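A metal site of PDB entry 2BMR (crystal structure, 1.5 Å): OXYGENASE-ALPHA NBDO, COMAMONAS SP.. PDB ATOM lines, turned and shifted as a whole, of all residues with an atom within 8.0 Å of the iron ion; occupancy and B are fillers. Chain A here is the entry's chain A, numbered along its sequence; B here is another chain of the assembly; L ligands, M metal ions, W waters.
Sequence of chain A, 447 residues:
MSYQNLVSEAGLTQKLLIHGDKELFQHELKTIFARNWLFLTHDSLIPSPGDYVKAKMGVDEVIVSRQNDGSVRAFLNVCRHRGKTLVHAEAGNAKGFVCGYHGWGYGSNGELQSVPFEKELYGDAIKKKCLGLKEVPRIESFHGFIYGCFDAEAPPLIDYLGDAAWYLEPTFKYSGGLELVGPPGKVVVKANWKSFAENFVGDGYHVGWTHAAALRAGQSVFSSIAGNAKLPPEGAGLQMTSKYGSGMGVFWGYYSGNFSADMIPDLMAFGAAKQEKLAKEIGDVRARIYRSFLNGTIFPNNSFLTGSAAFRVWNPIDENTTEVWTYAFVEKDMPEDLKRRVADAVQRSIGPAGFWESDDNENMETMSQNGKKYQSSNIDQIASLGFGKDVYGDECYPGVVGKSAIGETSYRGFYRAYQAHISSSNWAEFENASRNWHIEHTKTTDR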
ATOM      1  N   ASN A 199     -35.548 -27.987   8.709  1.00  0.00           N
ATOM      2  CA  ASN A 199     -34.406 -27.529   7.932  1.00  0.00           C
ATOM      3  C   ASN A 199     -34.834 -27.114   6.518  1.00  0.00           C
ATOM      4  O   ASN A 199     -34.471 -26.028   6.040  1.00  0.00           O
ATOM      5  CB  ASN A 199     -33.333 -28.616   7.900  1.00  0.00           C
ATOM      6  CG  ASN A 199     -32.101 -28.192   7.124  1.00  0.00           C
ATOM      7  OD1 ASN A 199     -31.995 -28.466   5.933  1.00  0.00           O
ATOM      8  ND2 ASN A 199     -31.192 -27.482   7.788  1.00  0.00           N
ATOM      9  N   PHE A 200     -35.638 -27.946   5.851  1.00  0.00           N
ATOM     10  CA  PHE A 200     -36.037 -27.614   4.486  1.00  0.00           C
ATOM     11  C   PHE A 200     -37.115 -26.543   4.409  1.00  0.00           C
ATOM     12  O   PHE A 200     -37.172 -25.811   3.403  1.00  0.00           O
ATOM     13  CB  PHE A 200     -36.408 -28.873   3.683  1.00  0.00           C
ATOM     14  CG  PHE A 200     -35.228 -29.506   3.010  1.00  0.00           C
ATOM     15  CD1 PHE A 200     -34.250 -30.124   3.787  1.00  0.00           C
ATOM     16  CD2 PHE A 200     -35.065 -29.435   1.638  1.00  0.00           C
ATOM     17  CE1 PHE A 200     -33.118 -30.682   3.187  1.00  0.00           C
ATOM     18  CE2 PHE A 200     -33.939 -30.009   1.021  1.00  0.00           C
ATOM     19  CZ  PHE A 200     -32.969 -30.624   1.803  1.00  0.00           C
ATOM     20  N   ASP A 203     -34.577 -23.134   6.475  1.00  0.00           N
ATOM     21  CA  ASP A 203     -33.208 -22.921   6.970  1.00  0.00           C
ATOM     22  C   ASP A 203     -32.213 -22.335   5.953  1.00  0.00           C
ATOM     23  O   ASP A 203     -31.219 -22.979   5.603  1.00  0.00           O
ATOM     24  CB  ASP A 203     -32.643 -24.179   7.621  1.00  0.00           C
ATOM     25  CG  ASP A 203     -31.542 -23.861   8.644  1.00  0.00           C
ATOM     26  OD1 ASP A 203     -31.241 -24.755   9.468  1.00  0.00           O
ATOM     27  OD2 ASP A 203     -31.005 -22.741   8.632  1.00  0.00           O
ATOM     28  N   HIS A 206     -28.500 -21.855   7.716  1.00  0.00           N
ATOM     29  CA  HIS A 206     -27.456 -22.883   7.901  1.00  0.00           C
ATOM     30  C   HIS A 206     -26.491 -22.966   6.733  1.00  0.00           C
ATOM     31  O   HIS A 206     -25.354 -23.416   6.898  1.00  0.00           O
ATOM     32  CB  HIS A 206     -28.069 -24.287   8.199  1.00  0.00           C
ATOM     33  CG  HIS A 206     -28.329 -25.139   6.986  1.00  0.00           C
ATOM     34  ND1 HIS A 206     -29.352 -24.880   6.086  1.00  0.00           N
ATOM     35  CD2 HIS A 206     -27.755 -26.293   6.574  1.00  0.00           C
ATOM     36  CE1 HIS A 206     -29.362 -25.828   5.152  1.00  0.00           C
ATOM     37  NE2 HIS A 206     -28.406 -26.693   5.433  1.00  0.00           N
ATOM     38  N   VAL A 207     -26.949 -22.561   5.553  1.00  0.00           N
ATOM     39  CA  VAL A 207     -26.211 -22.818   4.322  1.00  0.00           C
ATOM     40  C   VAL A 207     -24.766 -22.318   4.387  1.00  0.00           C
ATOM     41  O   VAL A 207     -23.826 -23.080   4.135  1.00  0.00           O
ATOM     42  CB  VAL A 207     -26.926 -22.224   3.093  1.00  0.00           C
ATOM     43  CG1 VAL A 207     -26.106 -22.454   1.817  1.00  0.00           C
ATOM     44  CG2 VAL A 207     -28.326 -22.827   2.966  1.00  0.00           C
ATOM     45  N   THR A 210     -22.970 -24.393   7.955  1.00  0.00           N
ATOM     46  CA  THR A 210     -22.898 -25.856   7.837  1.00  0.00           C
ATOM     47  C   THR A 210     -22.138 -26.280   6.564  1.00  0.00           C
ATOM     48  O   THR A 210     -21.299 -27.180   6.608  1.00  0.00           O
ATOM     49  CB  THR A 210     -24.316 -26.472   7.818  1.00  0.00           C
ATOM     50  OG1 THR A 210     -24.891 -26.419   9.138  1.00  0.00           O
ATOM     51  CG2 THR A 210     -24.282 -27.924   7.350  1.00  0.00           C
ATOM     52  N   HIS A 211     -22.442 -25.603   5.455  1.00  0.00           N
ATOM     53  CA  HIS A 211     -21.934 -26.017   4.146  1.00  0.00           C
ATOM     54  C   HIS A 211     -20.761 -25.150   3.662  1.00  0.00           C
ATOM     55  O   HIS A 211     -20.445 -25.143   2.469  1.00  0.00           O
ATOM     56  CB  HIS A 211     -23.077 -26.050   3.126  1.00  0.00           C
ATOM     57  CG  HIS A 211     -24.158 -27.017   3.484  1.00  0.00           C
ATOM     58  ND1 HIS A 211     -23.932 -28.364   3.631  1.00  0.00           N
ATOM     59  CD2 HIS A 211     -25.486 -26.829   3.718  1.00  0.00           C
ATOM     60  CE1 HIS A 211     -25.059 -28.970   3.964  1.00  0.00           C
ATOM     61  NE2 HIS A 211     -26.022 -28.057   4.029  1.00  0.00           N
ATOM     62  N   ASN A 258     -27.831 -25.620  -5.064  1.00  0.00           N
ATOM     63  CA  ASN A 258     -26.677 -26.267  -4.422  1.00  0.00           C
ATOM     64  C   ASN A 258     -25.773 -27.015  -5.405  1.00  0.00           C
ATOM     65  O   ASN A 258     -24.894 -27.781  -4.996  1.00  0.00           O
ATOM     66  CB  ASN A 258     -27.114 -27.169  -3.239  1.00  0.00           C
ATOM     67  CG  ASN A 258     -27.961 -28.350  -3.669  1.00  0.00           C
ATOM     68  OD1 ASN A 258     -27.888 -28.822  -4.798  1.00  0.00           O
ATOM     69  ND2 ASN A 258     -28.773 -28.848  -2.729  1.00  0.00           N
ATOM     70  N   LEU A 305     -36.551 -28.518  -3.185  1.00  0.00           N
ATOM     71  CA  LEU A 305     -35.773 -27.376  -3.616  1.00  0.00           C
ATOM     72  C   LEU A 305     -36.116 -27.150  -5.079  1.00  0.00           C
ATOM     73  O   LEU A 305     -36.180 -28.099  -5.852  1.00  0.00           O
ATOM     74  CB  LEU A 305     -34.275 -27.639  -3.512  1.00  0.00           C
ATOM     75  CG  LEU A 305     -33.749 -28.121  -2.160  1.00  0.00           C
ATOM     76  CD1 LEU A 305     -32.250 -28.412  -2.257  1.00  0.00           C
ATOM     77  CD2 LEU A 305     -34.043 -27.122  -1.048  1.00  0.00           C
ATOM     78  N   ARG A 312     -38.157 -34.481  -1.827  1.00  0.00           N
ATOM     79  CA  ARG A 312     -37.740 -35.328  -0.702  1.00  0.00           C
ATOM     80  C   ARG A 312     -38.902 -35.779   0.115  1.00  0.00           C
ATOM     81  O   ARG A 312     -39.902 -35.079   0.262  1.00  0.00           O
ATOM     82  CB  ARG A 312     -36.757 -34.579   0.192  1.00  0.00           C
ATOM     83  CG  ARG A 312     -35.832 -33.782  -0.677  1.00  0.00           C
ATOM     84  CD  ARG A 312     -34.456 -33.693  -0.195  1.00  0.00           C
ATOM     85  NE  ARG A 312     -33.809 -34.958   0.104  1.00  0.00           N
ATOM     86  CZ  ARG A 312     -32.721 -34.994   0.846  1.00  0.00           C
ATOM     87  NH1 ARG A 312     -32.250 -33.842   1.323  1.00  0.00           N
ATOM     88  NH2 ARG A 312     -32.103 -36.134   1.126  1.00  0.00           N
ATOM     89  N   SER A 349     -25.226 -33.663  -4.494  1.00  0.00           N
ATOM     90  CA  SER A 349     -25.293 -32.751  -3.359  1.00  0.00           C
ATOM     91  C   SER A 349     -26.028 -33.334  -2.173  1.00  0.00           C
ATOM     92  O   SER A 349     -25.538 -33.269  -1.043  1.00  0.00           O
ATOM     93  CB  SER A 349     -25.905 -31.394  -3.749  1.00  0.00           C
ATOM     94  OG  SER A 349     -24.990 -30.651  -4.531  1.00  0.00           O
ATOM     95  N   ILE A 350     -27.221 -33.883  -2.402  1.00  0.00           N
ATOM     96  CA  ILE A 350     -28.080 -34.231  -1.265  1.00  0.00           C
ATOM     97  C   ILE A 350     -28.605 -35.674  -1.223  1.00  0.00           C
ATOM     98  O   ILE A 350     -29.439 -35.998  -0.373  1.00  0.00           O
ATOM     99  CB  ILE A 350     -29.247 -33.229  -1.085  1.00  0.00           C
ATOM    100  CG1 ILE A 350     -30.165 -33.268  -2.309  1.00  0.00           C
ATOM    101  CG2 ILE A 350     -28.717 -31.824  -0.808  1.00  0.00           C
ATOM    102  CD1 ILE A 350     -31.434 -32.435  -2.162  1.00  0.00           C
ATOM    103  N   TRP A 356     -23.111 -32.349   0.350  1.00  0.00           N
ATOM    104  CA  TRP A 356     -23.808 -31.391   1.221  1.00  0.00           C
ATOM    105  C   TRP A 356     -24.575 -32.134   2.303  1.00  0.00           C
ATOM    106  O   TRP A 356     -24.416 -31.865   3.491  1.00  0.00           O
ATOM    107  CB  TRP A 356     -24.792 -30.545   0.420  1.00  0.00           C
ATOM    108  CG  TRP A 356     -24.177 -29.536  -0.513  1.00  0.00           C
ATOM    109  CD1 TRP A 356     -23.247 -29.771  -1.486  1.00  0.00           C
ATOM    110  CD2 TRP A 356     -24.519 -28.149  -0.591  1.00  0.00           C
ATOM    111  NE1 TRP A 356     -22.961 -28.593  -2.159  1.00  0.00           N
ATOM    112  CE2 TRP A 356     -23.717 -27.583  -1.618  1.00  0.00           C
ATOM    113  CE3 TRP A 356     -25.389 -27.319   0.123  1.00  0.00           C
ATOM    114  CZ2 TRP A 356     -23.789 -26.223  -1.971  1.00  0.00           C
ATOM    115  CZ3 TRP A 356     -25.442 -25.967  -0.217  1.00  0.00           C
ATOM    116  CH2 TRP A 356     -24.662 -25.435  -1.257  1.00  0.00           C
ATOM    117  N   GLU A 357     -25.429 -33.080   1.900  1.00  0.00           N
ATOM    118  CA  GLU A 357     -26.281 -33.795   2.847  1.00  0.00           C
ATOM    119  C   GLU A 357     -25.484 -34.429   3.994  1.00  0.00           C
ATOM    120  O   GLU A 357     -25.974 -34.500   5.120  1.00  0.00           O
ATOM    121  CB  GLU A 357     -27.165 -34.824   2.136  1.00  0.00           C
ATOM    122  CG  GLU A 357     -28.206 -35.507   3.070  1.00  0.00           C
ATOM    123  CD  GLU A 357     -29.642 -35.001   2.922  1.00  0.00           C
ATOM    124  OE1 GLU A 357     -29.883 -33.851   2.482  1.00  0.00           O
ATOM    125  OE2 GLU A 357     -30.554 -35.776   3.254  1.00  0.00           O
ATOM    126  N   SER A 358     -24.270 -34.901   3.699  1.00  0.00           N
ATOM    127  CA  SER A 358     -23.416 -35.462   4.743  1.00  0.00           C
ATOM    128  C   SER A 358     -23.252 -34.443   5.875  1.00  0.00           C
ATOM    129  O   SER A 358     -23.413 -34.786   7.052  1.00  0.00           O
ATOM    130  CB  SER A 358     -22.041 -35.852   4.195  1.00  0.00           C
ATOM    131  OG  SER A 358     -21.076 -35.963   5.223  1.00  0.00           O
ATOM    132  N   ASP A 359     -22.970 -33.192   5.500  1.00  0.00           N
ATOM    133  CA  ASP A 359     -22.741 -32.105   6.486  1.00  0.00           C
ATOM    134  C   ASP A 359     -23.923 -32.075   7.450  1.00  0.00           C
ATOM    135  O   ASP A 359     -23.760 -31.905   8.660  1.00  0.00           O
ATOM    136  CB  ASP A 359     -22.616 -30.728   5.803  1.00  0.00           C
ATOM    137  CG  ASP A 359     -21.411 -30.604   4.861  1.00  0.00           C
ATOM    138  OD1 ASP A 359     -21.538 -29.837   3.863  1.00  0.00           O
ATOM    139  OD2 ASP A 359     -20.344 -31.217   5.109  1.00  0.00           O
ATOM    140  N   ASP A 360     -25.121 -32.260   6.889  1.00  0.00           N
ATOM    141  CA  ASP A 360     -26.368 -32.113   7.642  1.00  0.00           C
ATOM    142  C   ASP A 360     -26.642 -33.206   8.649  1.00  0.00           C
ATOM    143  O   ASP A 360     -27.313 -32.958   9.672  1.00  0.00           O
ATOM    144  CB  ASP A 360     -27.546 -32.014   6.682  1.00  0.00           C
ATOM    145  CG  ASP A 360     -27.559 -30.719   5.921  1.00  0.00           C
ATOM    146  OD1 ASP A 360     -27.504 -29.650   6.580  1.00  0.00           O
ATOM    147  OD2 ASP A 360     -27.628 -30.762   4.683  1.00  0.00           O
ATOM    148  N   ASN A 361     -26.126 -34.403   8.398  1.00  0.00           N
ATOM    149  CA  ASN A 361     -26.383 -35.559   9.264  1.00  0.00           C
ATOM    150  C   ASN A 361     -26.274 -35.195  10.730  1.00  0.00           C
ATOM    151  O   ASN A 361     -27.182 -35.455  11.493  1.00  0.00           O
ATOM    152  CB  ASN A 361     -25.430 -36.724   8.995  1.00  0.00           C
ATOM    153  CG  ASN A 361     -25.789 -37.554   7.776  1.00  0.00           C
ATOM    154  OD1 ASN A 361     -25.042 -38.483   7.432  1.00  0.00           O
ATOM    155  ND2 ASN A 361     -26.902 -37.240   7.117  1.00  0.00           N
ATOM    156  N   ASN A 363     -26.168 -32.353  12.311  1.00  0.00           N
ATOM    157  CA  ASN A 363     -27.154 -31.358  12.752  1.00  0.00           C
ATOM    158  C   ASN A 363     -28.449 -32.047  13.148  1.00  0.00           C
ATOM    159  O   ASN A 363     -28.923 -31.857  14.263  1.00  0.00           O
ATOM    160  CB  ASN A 363     -27.423 -30.294  11.664  1.00  0.00           C
ATOM    161  CG  ASN A 363     -26.182 -29.487  11.310  1.00  0.00           C
ATOM    162  OD1 ASN A 363     -25.218 -29.399  12.082  1.00  0.00           O
ATOM    163  ND2 ASN A 363     -26.192 -28.891  10.116  1.00  0.00           N
ATOM    164  N   MET A 364     -28.986 -32.837  12.218  1.00  0.00           N
ATOM    165  CA  MET A 364     -30.275 -33.517  12.399  1.00  0.00           C
ATOM    166  C   MET A 364     -30.209 -34.570  13.502  1.00  0.00           C
ATOM    167  O   MET A 364     -31.090 -34.647  14.369  1.00  0.00           O
ATOM    168  CB  MET A 364     -30.692 -34.191  11.085  1.00  0.00           C
ATOM    169  CG  MET A 364     -30.705 -33.319   9.826  1.00  0.00           C
ATOM    170  SD  MET A 364     -32.024 -32.100   9.893  1.00  0.00           S
ATOM    171  CE  MET A 364     -31.183 -30.685  10.622  1.00  0.00           C
ATOM    172  N   TYR B 101     -23.878 -25.707  13.276  1.00  0.00           N
ATOM    173  CA  TYR B 101     -25.130 -25.625  12.511  1.00  0.00           C
ATOM    174  C   TYR B 101     -25.261 -24.233  11.859  1.00  0.00           C
ATOM    175  O   TYR B 101     -25.175 -24.123  10.629  1.00  0.00           O
ATOM    176  CB  TYR B 101     -26.333 -26.004  13.396  1.00  0.00           C
ATOM    177  CG  TYR B 101     -27.603 -26.446  12.655  1.00  0.00           C
ATOM    178  CD1 TYR B 101     -28.653 -27.046  13.367  1.00  0.00           C
ATOM    179  CD2 TYR B 101     -27.768 -26.256  11.281  1.00  0.00           C
ATOM    180  CE1 TYR B 101     -29.847 -27.432  12.722  1.00  0.00           C
ATOM    181  CE2 TYR B 101     -28.968 -26.658  10.618  1.00  0.00           C
ATOM    182  CZ  TYR B 101     -29.984 -27.244  11.352  1.00  0.00           C
ATOM    183  OH  TYR B 101     -31.161 -27.634  10.733  1.00  0.00           O
HETATM  184  C1  LIG L   1     -31.766 -24.646   2.119  1.00  0.00           C
HETATM  185  C2  LIG L   1     -30.843 -25.129   1.199  1.00  0.00           C
HETATM  186  C3  LIG L   1     -30.627 -26.506   1.076  1.00  0.00           C
HETATM  187  C4  LIG L   1     -31.336 -27.391   1.898  1.00  0.00           C
HETATM  188  C5  LIG L   1     -32.266 -26.897   2.821  1.00  0.00           C
HETATM  189  C6  LIG L   1     -32.474 -25.523   2.939  1.00  0.00           C
HETATM  190  C7  LIG L   1     -31.989 -23.160   2.248  1.00  0.00           C
HETATM  191  N1  LIG L   1     -29.722 -26.942   0.159  1.00  0.00           N
HETATM  192  O1  LIG L   1     -29.394 -26.167  -0.762  1.00  0.00           O
HETATM  193  O2  LIG L   1     -29.211 -28.073   0.209  1.00  0.00           O
HETATM  194 FE    FE M   1     -27.997 -28.540   4.475  1.00  0.00          FE
HETATM  195  O   HOH W   1     -29.961 -29.145   4.277  1.00  0.00           O
HETATM  196  O   HOH W   2     -28.087 -29.227   2.250  1.00  0.00           O
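The side-chain amide nitrogen of Asn 258 is in hydrogen-bond range of an oxygen (O2) of the ligand, 3.1 Å away.
A ring nitrogen (ND1) of His 211 lies within hydrogen-bond range of the side-chain carboxylate (OD1) of Asp 359.
ND1 of His 206 sits at hydrogen-bond distance from O of Asp 203, 2.7 Å away.
Within 4 Å of the iron ion: His 206, His 211 and Asp 360.
The iron ion is bound by water W1 (2.1 Å), a ring nitrogen (NE2) of His 211 (2.1 Å), a ring nitrogen (NE2) of His 206 (2.1 Å), the side-chain carboxylate (OD2) of Asp 360 (2.3 Å), water W2 (2.3 Å) and the side-chain carboxylate (OD1) of Asp 360 (2.4 Å).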
